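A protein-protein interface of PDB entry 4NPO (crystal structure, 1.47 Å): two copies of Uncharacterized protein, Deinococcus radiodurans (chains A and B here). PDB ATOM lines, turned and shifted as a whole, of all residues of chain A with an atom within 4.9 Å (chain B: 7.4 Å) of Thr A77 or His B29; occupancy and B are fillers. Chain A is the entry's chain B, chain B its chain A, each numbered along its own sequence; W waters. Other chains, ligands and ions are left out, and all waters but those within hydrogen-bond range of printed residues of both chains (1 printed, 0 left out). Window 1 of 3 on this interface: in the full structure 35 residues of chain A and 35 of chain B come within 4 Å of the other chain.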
ATOM      1  N   SER A  28     -20.216  -0.009 -22.513  1.00  0.00           N
ATOM      2  CA  SER A  28     -21.577   0.392 -22.132  1.00  0.00           C
ATOM      3  C   SER A  28     -22.173  -0.675 -21.248  1.00  0.00           C
ATOM      4  O   SER A  28     -22.004  -1.865 -21.486  1.00  0.00           O
ATOM      5  CB  SER A  28     -22.431   0.568 -23.327  1.00  0.00           C
ATOM      6  OG  SER A  28     -23.701   1.161 -23.056  1.00  0.00           O
ATOM      7  N   LEU A  61     -18.279  -6.270 -28.836  1.00  0.00           N
ATOM      8  CA  LEU A  61     -19.037  -7.115 -27.945  1.00  0.00           C
ATOM      9  C   LEU A  61     -20.423  -6.534 -27.769  1.00  0.00           C
ATOM     10  O   LEU A  61     -20.550  -5.357 -27.445  1.00  0.00           O
ATOM     11  CB  LEU A  61     -18.354  -7.222 -26.574  1.00  0.00           C
ATOM     12  CG  LEU A  61     -19.019  -8.208 -25.600  1.00  0.00           C
ATOM     13  CD1 LEU A  61     -18.692  -9.625 -26.040  1.00  0.00           C
ATOM     14  CD2 LEU A  61     -18.491  -7.979 -24.185  1.00  0.00           C
ATOM     15  N   TYR A  62     -21.469  -7.353 -27.873  1.00  0.00           N
ATOM     16  CA  TYR A  62     -22.788  -6.970 -27.495  1.00  0.00           C
ATOM     17  C   TYR A  62     -23.469  -8.167 -26.907  1.00  0.00           C
ATOM     18  O   TYR A  62     -23.870  -9.081 -27.647  1.00  0.00           O
ATOM     19  CB  TYR A  62     -23.543  -6.364 -28.685  1.00  0.00           C
ATOM     20  CG  TYR A  62     -24.761  -5.601 -28.309  1.00  0.00           C
ATOM     21  CD1 TYR A  62     -25.901  -6.230 -27.837  1.00  0.00           C
ATOM     22  CD2 TYR A  62     -24.772  -4.221 -28.350  1.00  0.00           C
ATOM     23  CE1 TYR A  62     -27.032  -5.504 -27.467  1.00  0.00           C
ATOM     24  CE2 TYR A  62     -25.883  -3.512 -27.970  1.00  0.00           C
ATOM     25  CZ  TYR A  62     -27.018  -4.160 -27.573  1.00  0.00           C
ATOM     26  OH  TYR A  62     -28.146  -3.435 -27.211  1.00  0.00           O
ATOM     27  N   LEU A  63     -23.491  -8.238 -25.597  1.00  0.00           N
ATOM     28  CA  LEU A  63     -23.941  -9.420 -24.876  1.00  0.00           C
ATOM     29  C   LEU A  63     -25.180  -9.015 -24.113  1.00  0.00           C
ATOM     30  O   LEU A  63     -25.189  -8.059 -23.360  1.00  0.00           O
ATOM     31  CB  LEU A  63     -22.853  -9.839 -23.936  1.00  0.00           C
ATOM     32  CG  LEU A  63     -22.722 -11.235 -23.412  1.00  0.00           C
ATOM     33  CD1 LEU A  63     -21.342 -11.332 -22.753  1.00  0.00           C
ATOM     34  CD2 LEU A  63     -23.782 -11.522 -22.403  1.00  0.00           C
ATOM     35  N   LEU A  75     -29.131  -7.491 -18.402  1.00  0.00           N
ATOM     36  CA  LEU A  75     -27.952  -6.678 -18.635  1.00  0.00           C
ATOM     37  C   LEU A  75     -27.672  -6.604 -20.107  1.00  0.00           C
ATOM     38  O   LEU A  75     -27.784  -7.594 -20.838  1.00  0.00           O
ATOM     39  CB  LEU A  75     -26.758  -7.277 -17.933  1.00  0.00           C
ATOM     40  CG  LEU A  75     -26.569  -7.161 -16.470  1.00  0.00           C
ATOM     41  CD1 LEU A  75     -27.605  -7.974 -15.777  1.00  0.00           C
ATOM     42  CD2 LEU A  75     -25.180  -7.613 -16.084  1.00  0.00           C
ATOM     43  N   ILE A  76     -27.217  -5.436 -20.538  1.00  0.00           N
ATOM     44  CA  ILE A  76     -26.763  -5.227 -21.892  1.00  0.00           C
ATOM     45  C   ILE A  76     -25.321  -4.768 -21.766  1.00  0.00           C
ATOM     46  O   ILE A  76     -25.052  -3.699 -21.188  1.00  0.00           O
ATOM     47  CB  ILE A  76     -27.559  -4.191 -22.661  1.00  0.00           C
ATOM     48  CG1 ILE A  76     -29.032  -4.549 -22.712  1.00  0.00           C
ATOM     49  CG2 ILE A  76     -26.990  -4.043 -24.054  1.00  0.00           C
ATOM     50  CD1 ILE A  76     -29.973  -3.513 -23.324  1.00  0.00           C
ATOM     51  N   THR A  77     -24.352  -5.556 -22.203  1.00  0.00           N
ATOM     52  CA  THR A  77     -22.931  -5.325 -22.037  1.00  0.00           C
ATOM     53  C   THR A  77     -22.344  -5.095 -23.408  1.00  0.00           C
ATOM     54  O   THR A  77     -22.413  -5.971 -24.276  1.00  0.00           O
ATOM     55  CB  THR A  77     -22.248  -6.539 -21.430  1.00  0.00           C
ATOM     56  OG1 THR A  77     -22.881  -6.728 -20.146  1.00  0.00           O
ATOM     57  CG2 THR A  77     -20.723  -6.381 -21.287  1.00  0.00           C
ATOM     58  N   GLU A  78     -21.797  -3.923 -23.646  1.00  0.00           N
ATOM     59  CA  GLU A  78     -21.287  -3.583 -24.977  1.00  0.00           C
ATOM     60  C   GLU A  78     -19.876  -3.104 -24.871  1.00  0.00           C
ATOM     61  O   GLU A  78     -19.524  -2.358 -23.946  1.00  0.00           O
ATOM     62  CB  GLU A  78     -22.093  -2.474 -25.611  1.00  0.00           C
ATOM     63  CG  GLU A  78     -23.582  -2.578 -25.369  1.00  0.00           C
ATOM     64  CD  GLU A  78     -24.395  -1.447 -25.911  1.00  0.00           C
ATOM     65  OE1 GLU A  78     -23.912  -0.686 -26.818  1.00  0.00           O
ATOM     66  OE2 GLU A  78     -25.516  -1.242 -25.409  1.00  0.00           O
ATOM     67  N   HIS A  79     -19.069  -3.479 -25.858  1.00  0.00           N
ATOM     68  CA  HIS A  79     -17.733  -2.921 -26.031  1.00  0.00           C
ATOM     69  C   HIS A  79     -17.659  -2.388 -27.445  1.00  0.00           C
ATOM     70  O   HIS A  79     -17.986  -3.115 -28.363  1.00  0.00           O
ATOM     71  CB  HIS A  79     -16.595  -3.941 -25.843  1.00  0.00           C
ATOM     72  CG  HIS A  79     -16.529  -4.536 -24.492  1.00  0.00           C
ATOM     73  ND1 HIS A  79     -15.616  -5.512 -24.186  1.00  0.00           N
ATOM     74  CD2 HIS A  79     -17.154  -4.215 -23.330  1.00  0.00           C
ATOM     75  CE1 HIS A  79     -15.731  -5.835 -22.917  1.00  0.00           C
ATOM     76  NE2 HIS A  79     -16.655  -5.067 -22.378  1.00  0.00           N
ATOM     77  N   ILE B  27     -13.812  -1.016 -14.105  1.00  0.00           N
ATOM     78  CA  ILE B  27     -14.792  -1.950 -14.562  1.00  0.00           C
ATOM     79  C   ILE B  27     -14.136  -3.253 -14.863  1.00  0.00           C
ATOM     80  O   ILE B  27     -13.089  -3.279 -15.504  1.00  0.00           O
ATOM     81  CB  ILE B  27     -15.458  -1.452 -15.837  1.00  0.00           C
ATOM     82  CG1 ILE B  27     -16.262  -0.257 -15.504  1.00  0.00           C
ATOM     83  CG2 ILE B  27     -16.348  -2.608 -16.380  1.00  0.00           C
ATOM     84  CD1 ILE B  27     -16.800   0.540 -16.689  1.00  0.00           C
ATOM     85  N   SER B  28     -14.635  -4.354 -14.347  1.00  0.00           N
ATOM     86  CA  SER B  28     -14.114  -5.658 -14.688  1.00  0.00           C
ATOM     87  C   SER B  28     -15.206  -6.393 -15.436  1.00  0.00           C
ATOM     88  O   SER B  28     -16.379  -6.410 -15.022  1.00  0.00           O
ATOM     89  CB  SER B  28     -13.794  -6.439 -13.434  1.00  0.00           C
ATOM     90  OG  SER B  28     -13.139  -7.708 -13.632  1.00  0.00           O
ATOM     91  N   HIS B  29     -14.779  -7.072 -16.473  1.00  0.00           N
ATOM     92  CA  HIS B  29     -15.629  -7.912 -17.283  1.00  0.00           C
ATOM     93  C   HIS B  29     -15.038  -9.305 -17.321  1.00  0.00           C
ATOM     94  O   HIS B  29     -13.906  -9.504 -17.760  1.00  0.00           O
ATOM     95  CB  HIS B  29     -15.544  -7.354 -18.703  1.00  0.00           C
ATOM     96  CG  HIS B  29     -16.205  -8.213 -19.709  1.00  0.00           C
ATOM     97  ND1 HIS B  29     -17.569  -8.264 -19.854  1.00  0.00           N
ATOM     98  CD2 HIS B  29     -15.698  -9.057 -20.634  1.00  0.00           C
ATOM     99  CE1 HIS B  29     -17.880  -9.133 -20.806  1.00  0.00           C
ATOM    100  NE2 HIS B  29     -16.763  -9.646 -21.274  1.00  0.00           N
ATOM    101  N   GLY B  30     -15.785 -10.294 -16.839  1.00  0.00           N
ATOM    102  CA  GLY B  30     -15.365 -11.672 -16.798  1.00  0.00           C
ATOM    103  C   GLY B  30     -16.282 -12.560 -17.558  1.00  0.00           C
ATOM    104  O   GLY B  30     -17.497 -12.376 -17.515  1.00  0.00           O
ATOM    105  N   THR B  31     -15.749 -13.548 -18.243  1.00  0.00           N
ATOM    106  CA  THR B  31     -16.535 -14.560 -18.895  1.00  0.00           C
ATOM    107  C   THR B  31     -16.057 -15.910 -18.578  1.00  0.00           C
ATOM    108  O   THR B  31     -14.847 -16.109 -18.295  1.00  0.00           O
ATOM    109  CB  THR B  31     -16.527 -14.386 -20.410  1.00  0.00           C
ATOM    110  OG1 THR B  31     -15.195 -14.374 -20.897  1.00  0.00           O
ATOM    111  CG2 THR B  31     -17.152 -13.064 -20.851  1.00  0.00           C
ATOM    112  N   SER B  65     -24.329 -13.012 -14.441  1.00  0.00           N
ATOM    113  CA  SER B  65     -25.428 -13.156 -15.387  1.00  0.00           C
ATOM    114  C   SER B  65     -25.126 -14.237 -16.381  1.00  0.00           C
ATOM    115  O   SER B  65     -24.001 -14.676 -16.554  1.00  0.00           O
ATOM    116  CB  SER B  65     -25.769 -11.813 -16.001  1.00  0.00           C
ATOM    117  OG  SER B  65     -24.683 -11.350 -16.802  1.00  0.00           O
ATOM    118  N   PHE B  74     -21.432 -17.469 -18.963  1.00  0.00           N
ATOM    119  CA  PHE B  74     -21.698 -16.541 -17.889  1.00  0.00           C
ATOM    120  C   PHE B  74     -20.828 -15.306 -17.959  1.00  0.00           C
ATOM    121  O   PHE B  74     -19.750 -15.312 -18.584  1.00  0.00           O
ATOM    122  CB  PHE B  74     -21.501 -17.224 -16.571  1.00  0.00           C
ATOM    123  CG  PHE B  74     -22.372 -18.430 -16.411  1.00  0.00           C
ATOM    124  CD1 PHE B  74     -23.702 -18.231 -16.069  1.00  0.00           C
ATOM    125  CD2 PHE B  74     -21.955 -19.711 -16.668  1.00  0.00           C
ATOM    126  CE1 PHE B  74     -24.561 -19.293 -15.998  1.00  0.00           C
ATOM    127  CE2 PHE B  74     -22.791 -20.750 -16.561  1.00  0.00           C
ATOM    128  CZ  PHE B  74     -24.125 -20.555 -16.220  1.00  0.00           C
ATOM    129  N   LEU B  75     -21.307 -14.220 -17.374  1.00  0.00           N
ATOM    130  CA  LEU B  75     -20.655 -12.964 -17.325  1.00  0.00           C
ATOM    131  C   LEU B  75     -20.566 -12.550 -15.886  1.00  0.00           C
ATOM    132  O   LEU B  75     -21.532 -12.618 -15.101  1.00  0.00           O
ATOM    133  CB  LEU B  75     -21.452 -11.935 -18.058  1.00  0.00           C
ATOM    134  CG  LEU B  75     -21.008 -10.460 -18.180  1.00  0.00           C
ATOM    135  CD1 LEU B  75     -19.723 -10.311 -18.901  1.00  0.00           C
ATOM    136  CD2 LEU B  75     -22.007  -9.505 -18.812  1.00  0.00           C
ATOM    137  N   ILE B  76     -19.429 -11.961 -15.534  1.00  0.00           N
ATOM    138  CA  ILE B  76     -19.193 -11.343 -14.246  1.00  0.00           C
ATOM    139  C   ILE B  76     -18.921  -9.890 -14.493  1.00  0.00           C
ATOM    140  O   ILE B  76     -17.935  -9.539 -15.172  1.00  0.00           O
ATOM    141  CB  ILE B  76     -18.037 -11.990 -13.467  1.00  0.00           C
ATOM    142  CG1 ILE B  76     -18.196 -13.507 -13.354  1.00  0.00           C
ATOM    143  CG2 ILE B  76     -17.960 -11.333 -12.106  1.00  0.00           C
ATOM    144  CD1 ILE B  76     -17.050 -14.182 -12.655  1.00  0.00           C
ATOM    145  N   THR B  77     -19.761  -9.011 -13.989  1.00  0.00           N
ATOM    146  CA  THR B  77     -19.668  -7.587 -14.211  1.00  0.00           C
ATOM    147  C   THR B  77     -19.385  -6.935 -12.882  1.00  0.00           C
ATOM    148  O   THR B  77     -20.150  -7.092 -11.932  1.00  0.00           O
ATOM    149  CB  THR B  77     -21.002  -7.025 -14.705  1.00  0.00           C
ATOM    150  OG1 THR B  77     -21.299  -7.671 -15.960  1.00  0.00           O
ATOM    151  CG2 THR B  77     -20.960  -5.543 -14.849  1.00  0.00           C
ATOM    152  N   GLU B  78     -18.262  -6.243 -12.765  1.00  0.00           N
ATOM    153  CA  GLU B  78     -17.866  -5.678 -11.496  1.00  0.00           C
ATOM    154  C   GLU B  78     -17.499  -4.231 -11.706  1.00  0.00           C
ATOM    155  O   GLU B  78     -16.861  -3.892 -12.674  1.00  0.00           O
ATOM    156  CB  GLU B  78     -16.650  -6.365 -10.882  1.00  0.00           C
ATOM    157  CG  GLU B  78     -16.642  -7.861 -11.095  1.00  0.00           C
ATOM    158  CD  GLU B  78     -15.402  -8.542 -10.577  1.00  0.00           C
ATOM    159  OE1 GLU B  78     -14.684  -8.011  -9.719  1.00  0.00           O
ATOM    160  OE2 GLU B  78     -15.125  -9.669 -11.048  1.00  0.00           O
ATOM    161  N   MET B  86     -10.076  -3.386  -6.147  1.00  0.00           N
ATOM    162  CA  MET B  86     -10.170  -4.600  -6.914  1.00  0.00           C
ATOM    163  C   MET B  86      -9.016  -5.542  -6.560  1.00  0.00           C
ATOM    164  O   MET B  86      -9.216  -6.739  -6.401  1.00  0.00           O
ATOM    165  CB  MET B  86     -10.177  -4.305  -8.401  1.00  0.00           C
ATOM    166  CG  MET B  86     -10.462  -5.564  -9.153  1.00  0.00           C
ATOM    167  SD  MET B  86     -10.469  -5.249 -10.903  1.00  0.00           S
ATOM    168  CE  MET B  86      -8.786  -5.024 -11.215  1.00  0.00           C
ATOM    169  N   LEU B 110     -12.179 -19.176 -17.579  1.00  0.00           N
ATOM    170  CA  LEU B 110     -12.426 -17.906 -16.910  1.00  0.00           C
ATOM    171  C   LEU B 110     -11.473 -16.865 -17.442  1.00  0.00           C
ATOM    172  O   LEU B 110     -10.237 -17.055 -17.299  1.00  0.00           O
ATOM    173  CB  LEU B 110     -12.312 -18.008 -15.409  1.00  0.00           C
ATOM    174  CG  LEU B 110     -12.424 -16.718 -14.620  1.00  0.00           C
ATOM    175  CD1 LEU B 110     -13.760 -16.087 -14.835  1.00  0.00           C
ATOM    176  CD2 LEU B 110     -12.182 -17.011 -13.147  1.00  0.00           C
ATOM    177  N   LYS B 111     -11.960 -15.772 -17.994  1.00  0.00           N
ATOM    178  CA  LYS B 111     -11.186 -14.700 -18.473  1.00  0.00           C
ATOM    179  C   LYS B 111     -11.712 -13.409 -17.872  1.00  0.00           C
ATOM    180  O   LYS B 111     -12.925 -13.164 -17.994  1.00  0.00           O
ATOM    181  CB  LYS B 111     -11.275 -14.610 -19.982  1.00  0.00           C
ATOM    182  CG  LYS B 111     -10.400 -13.526 -20.548  1.00  0.00           C
ATOM    183  CD  LYS B 111     -10.444 -13.530 -22.055  1.00  0.00           C
ATOM    184  CE  LYS B 111      -9.813 -12.289 -22.652  1.00  0.00           C
ATOM    185  NZ  LYS B 111      -8.404 -12.138 -22.233  1.00  0.00           N
ATOM    186  N   ILE B 112     -10.865 -12.632 -17.243  1.00  0.00           N
ATOM    187  CA  ILE B 112     -11.247 -11.402 -16.595  1.00  0.00           C
ATOM    188  C   ILE B 112     -10.348 -10.305 -17.095  1.00  0.00           C
ATOM    189  O   ILE B 112      -9.100 -10.470 -17.095  1.00  0.00           O
ATOM    190  CB  ILE B 112     -11.151 -11.543 -15.092  1.00  0.00           C
ATOM    191  CG1 ILE B 112     -12.034 -12.717 -14.608  1.00  0.00           C
ATOM    192  CG2 ILE B 112     -11.522 -10.269 -14.389  1.00  0.00           C
ATOM    193  CD1 ILE B 112     -11.868 -12.986 -13.165  1.00  0.00           C
ATOM    194  N   THR B 113     -10.968  -9.221 -17.523  1.00  0.00           N
ATOM    195  CA  THR B 113     -10.280  -8.027 -18.011  1.00  0.00           C
ATOM    196  C   THR B 113     -10.801  -6.874 -17.253  1.00  0.00           C
ATOM    197  O   THR B 113     -12.024  -6.723 -17.112  1.00  0.00           O
ATOM    198  CB  THR B 113     -10.487  -7.817 -19.501  1.00  0.00           C
ATOM    199  OG1 THR B 113     -10.132  -9.002 -20.181  1.00  0.00           O
ATOM    200  CG2 THR B 113      -9.599  -6.709 -20.010  1.00  0.00           C
ATOM    201  N   ALA B 114      -9.926  -6.008 -16.745  1.00  0.00           N
ATOM    202  CA  ALA B 114     -10.330  -4.823 -16.017  1.00  0.00           C
ATOM    203  C   ALA B 114      -9.958  -3.583 -16.796  1.00  0.00           C
ATOM    204  O   ALA B 114      -9.046  -3.626 -17.613  1.00  0.00           O
ATOM    205  CB  ALA B 114      -9.679  -4.789 -14.669  1.00  0.00           C
ATOM    206  N   TYR B 115     -10.747  -2.546 -16.643  1.00  0.00           N
ATOM    207  CA  TYR B 115     -10.538  -1.303 -17.379  1.00  0.00           C
ATOM    208  C   TYR B 115     -10.722  -0.128 -16.439  1.00  0.00           C
ATOM    209  O   TYR B 115     -11.623  -0.061 -15.616  1.00  0.00           O
ATOM    210  CB  TYR B 115     -11.602  -1.173 -18.456  1.00  0.00           C
ATOM    211  CG  TYR B 115     -11.684  -2.306 -19.436  1.00  0.00           C
ATOM    212  CD1 TYR B 115     -12.458  -3.399 -19.132  1.00  0.00           C
ATOM    213  CD2 TYR B 115     -10.975  -2.302 -20.616  1.00  0.00           C
ATOM    214  CE1 TYR B 115     -12.579  -4.443 -20.023  1.00  0.00           C
ATOM    215  CE2 TYR B 115     -11.063  -3.364 -21.481  1.00  0.00           C
ATOM    216  CZ  TYR B 115     -11.872  -4.414 -21.152  1.00  0.00           C
ATOM    217  OH  TYR B 115     -11.986  -5.476 -22.049  1.00  0.00           O
HETATM  218  O   HOH W   1     -22.140  -5.187 -18.185  1.00  0.00           O
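O of Ile B27 lies within hydrogen-bond range of N of Tyr B115.
O of Ser B65 sits at hydrogen-bond distance from N of Leu B75 (2.9 Å).
N of His B29 is in hydrogen-bond range of O of Thr B113 (2.8 Å).
O of Thr A77 sits at hydrogen-bond distance from N of Leu A63.
The backbone carbonyl oxygen (O) of Leu A61 sits at hydrogen-bond distance from the backbone NH (N) of His A79.
Among the printed residues, merely in contact across the chains: Leu A61 with His B29 (3.6 Å), Leu A75 with Ser B65 (3.8 Å), Leu A75 with Thr B77 (3.9 Å), Thr A77 with His B29 (3.9 Å), Thr A77 with Leu B75 (3.2 Å), His A79 with His B29 (3.9 Å) and His A79 with Tyr B115 (3.9 Å).
Of the printed residues of chain B, Thr A77 touches His B29 (3.9 Å) and Leu B75 (3.2 Å).
Printed residues of chain A within 4 Å of His B29: Leu A61 (3.6 Å), Thr A77 (3.9 Å) and His A79 (3.9 Å).
Of the printed residues of chain B, Leu A61 touches His B29 (3.6 Å).
Of the printed residues of chain B, His A79 touches His B29 and Tyr B115.
Of the printed residues of chain A, Thr B77 touches Leu A75.
Of the printed residues of chain B, Leu A75 touches Ser B65 (3.8 Å) and Thr B77 (3.9 Å).
Printed residues of chain A within 4 Å of Tyr B115: His A79.
Glu B78 touches none of the printed residues of chain A.
The nearest printed residue of chain B that does not touch Thr A77 is Thr B77 (4.6 Å).
The nearest printed residue of chain A that does not touch His B29 is Leu A63 (4.5 Å).
Of the 18 printed residues of chain B, 5 touch a printed residue of chain A.
Hydrophobic or aromatic side chains of chain B within 4 Å of the printed part of chain A: His B29, Leu B75 and Tyr B115.
Along chain B the printed residues that touch a printed residue of chain A span positions 29 to 115.
Hydrophobic or aromatic side chains of chain A within 4 Å of the printed part of chain B: Leu A61, Leu A75 and His A79.
Among the printed residues, no Asp or Glu carboxylate lies within 4 Å of a Lys or Arg side-chain nitrogen of the other chain.
Leu A75 touches Thr B77, and with the chains exchanged Thr A77 touches Leu B75.
Positions printed for both chains: 28, 75, 76, 77 and 78.
Water W1 lies within hydrogen-bond range of the side-chain hydroxyl (OG1) of Thr A77 (2.6 Å) and the side-chain hydroxyl (OG1) of Thr B77 (3.4 Å).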
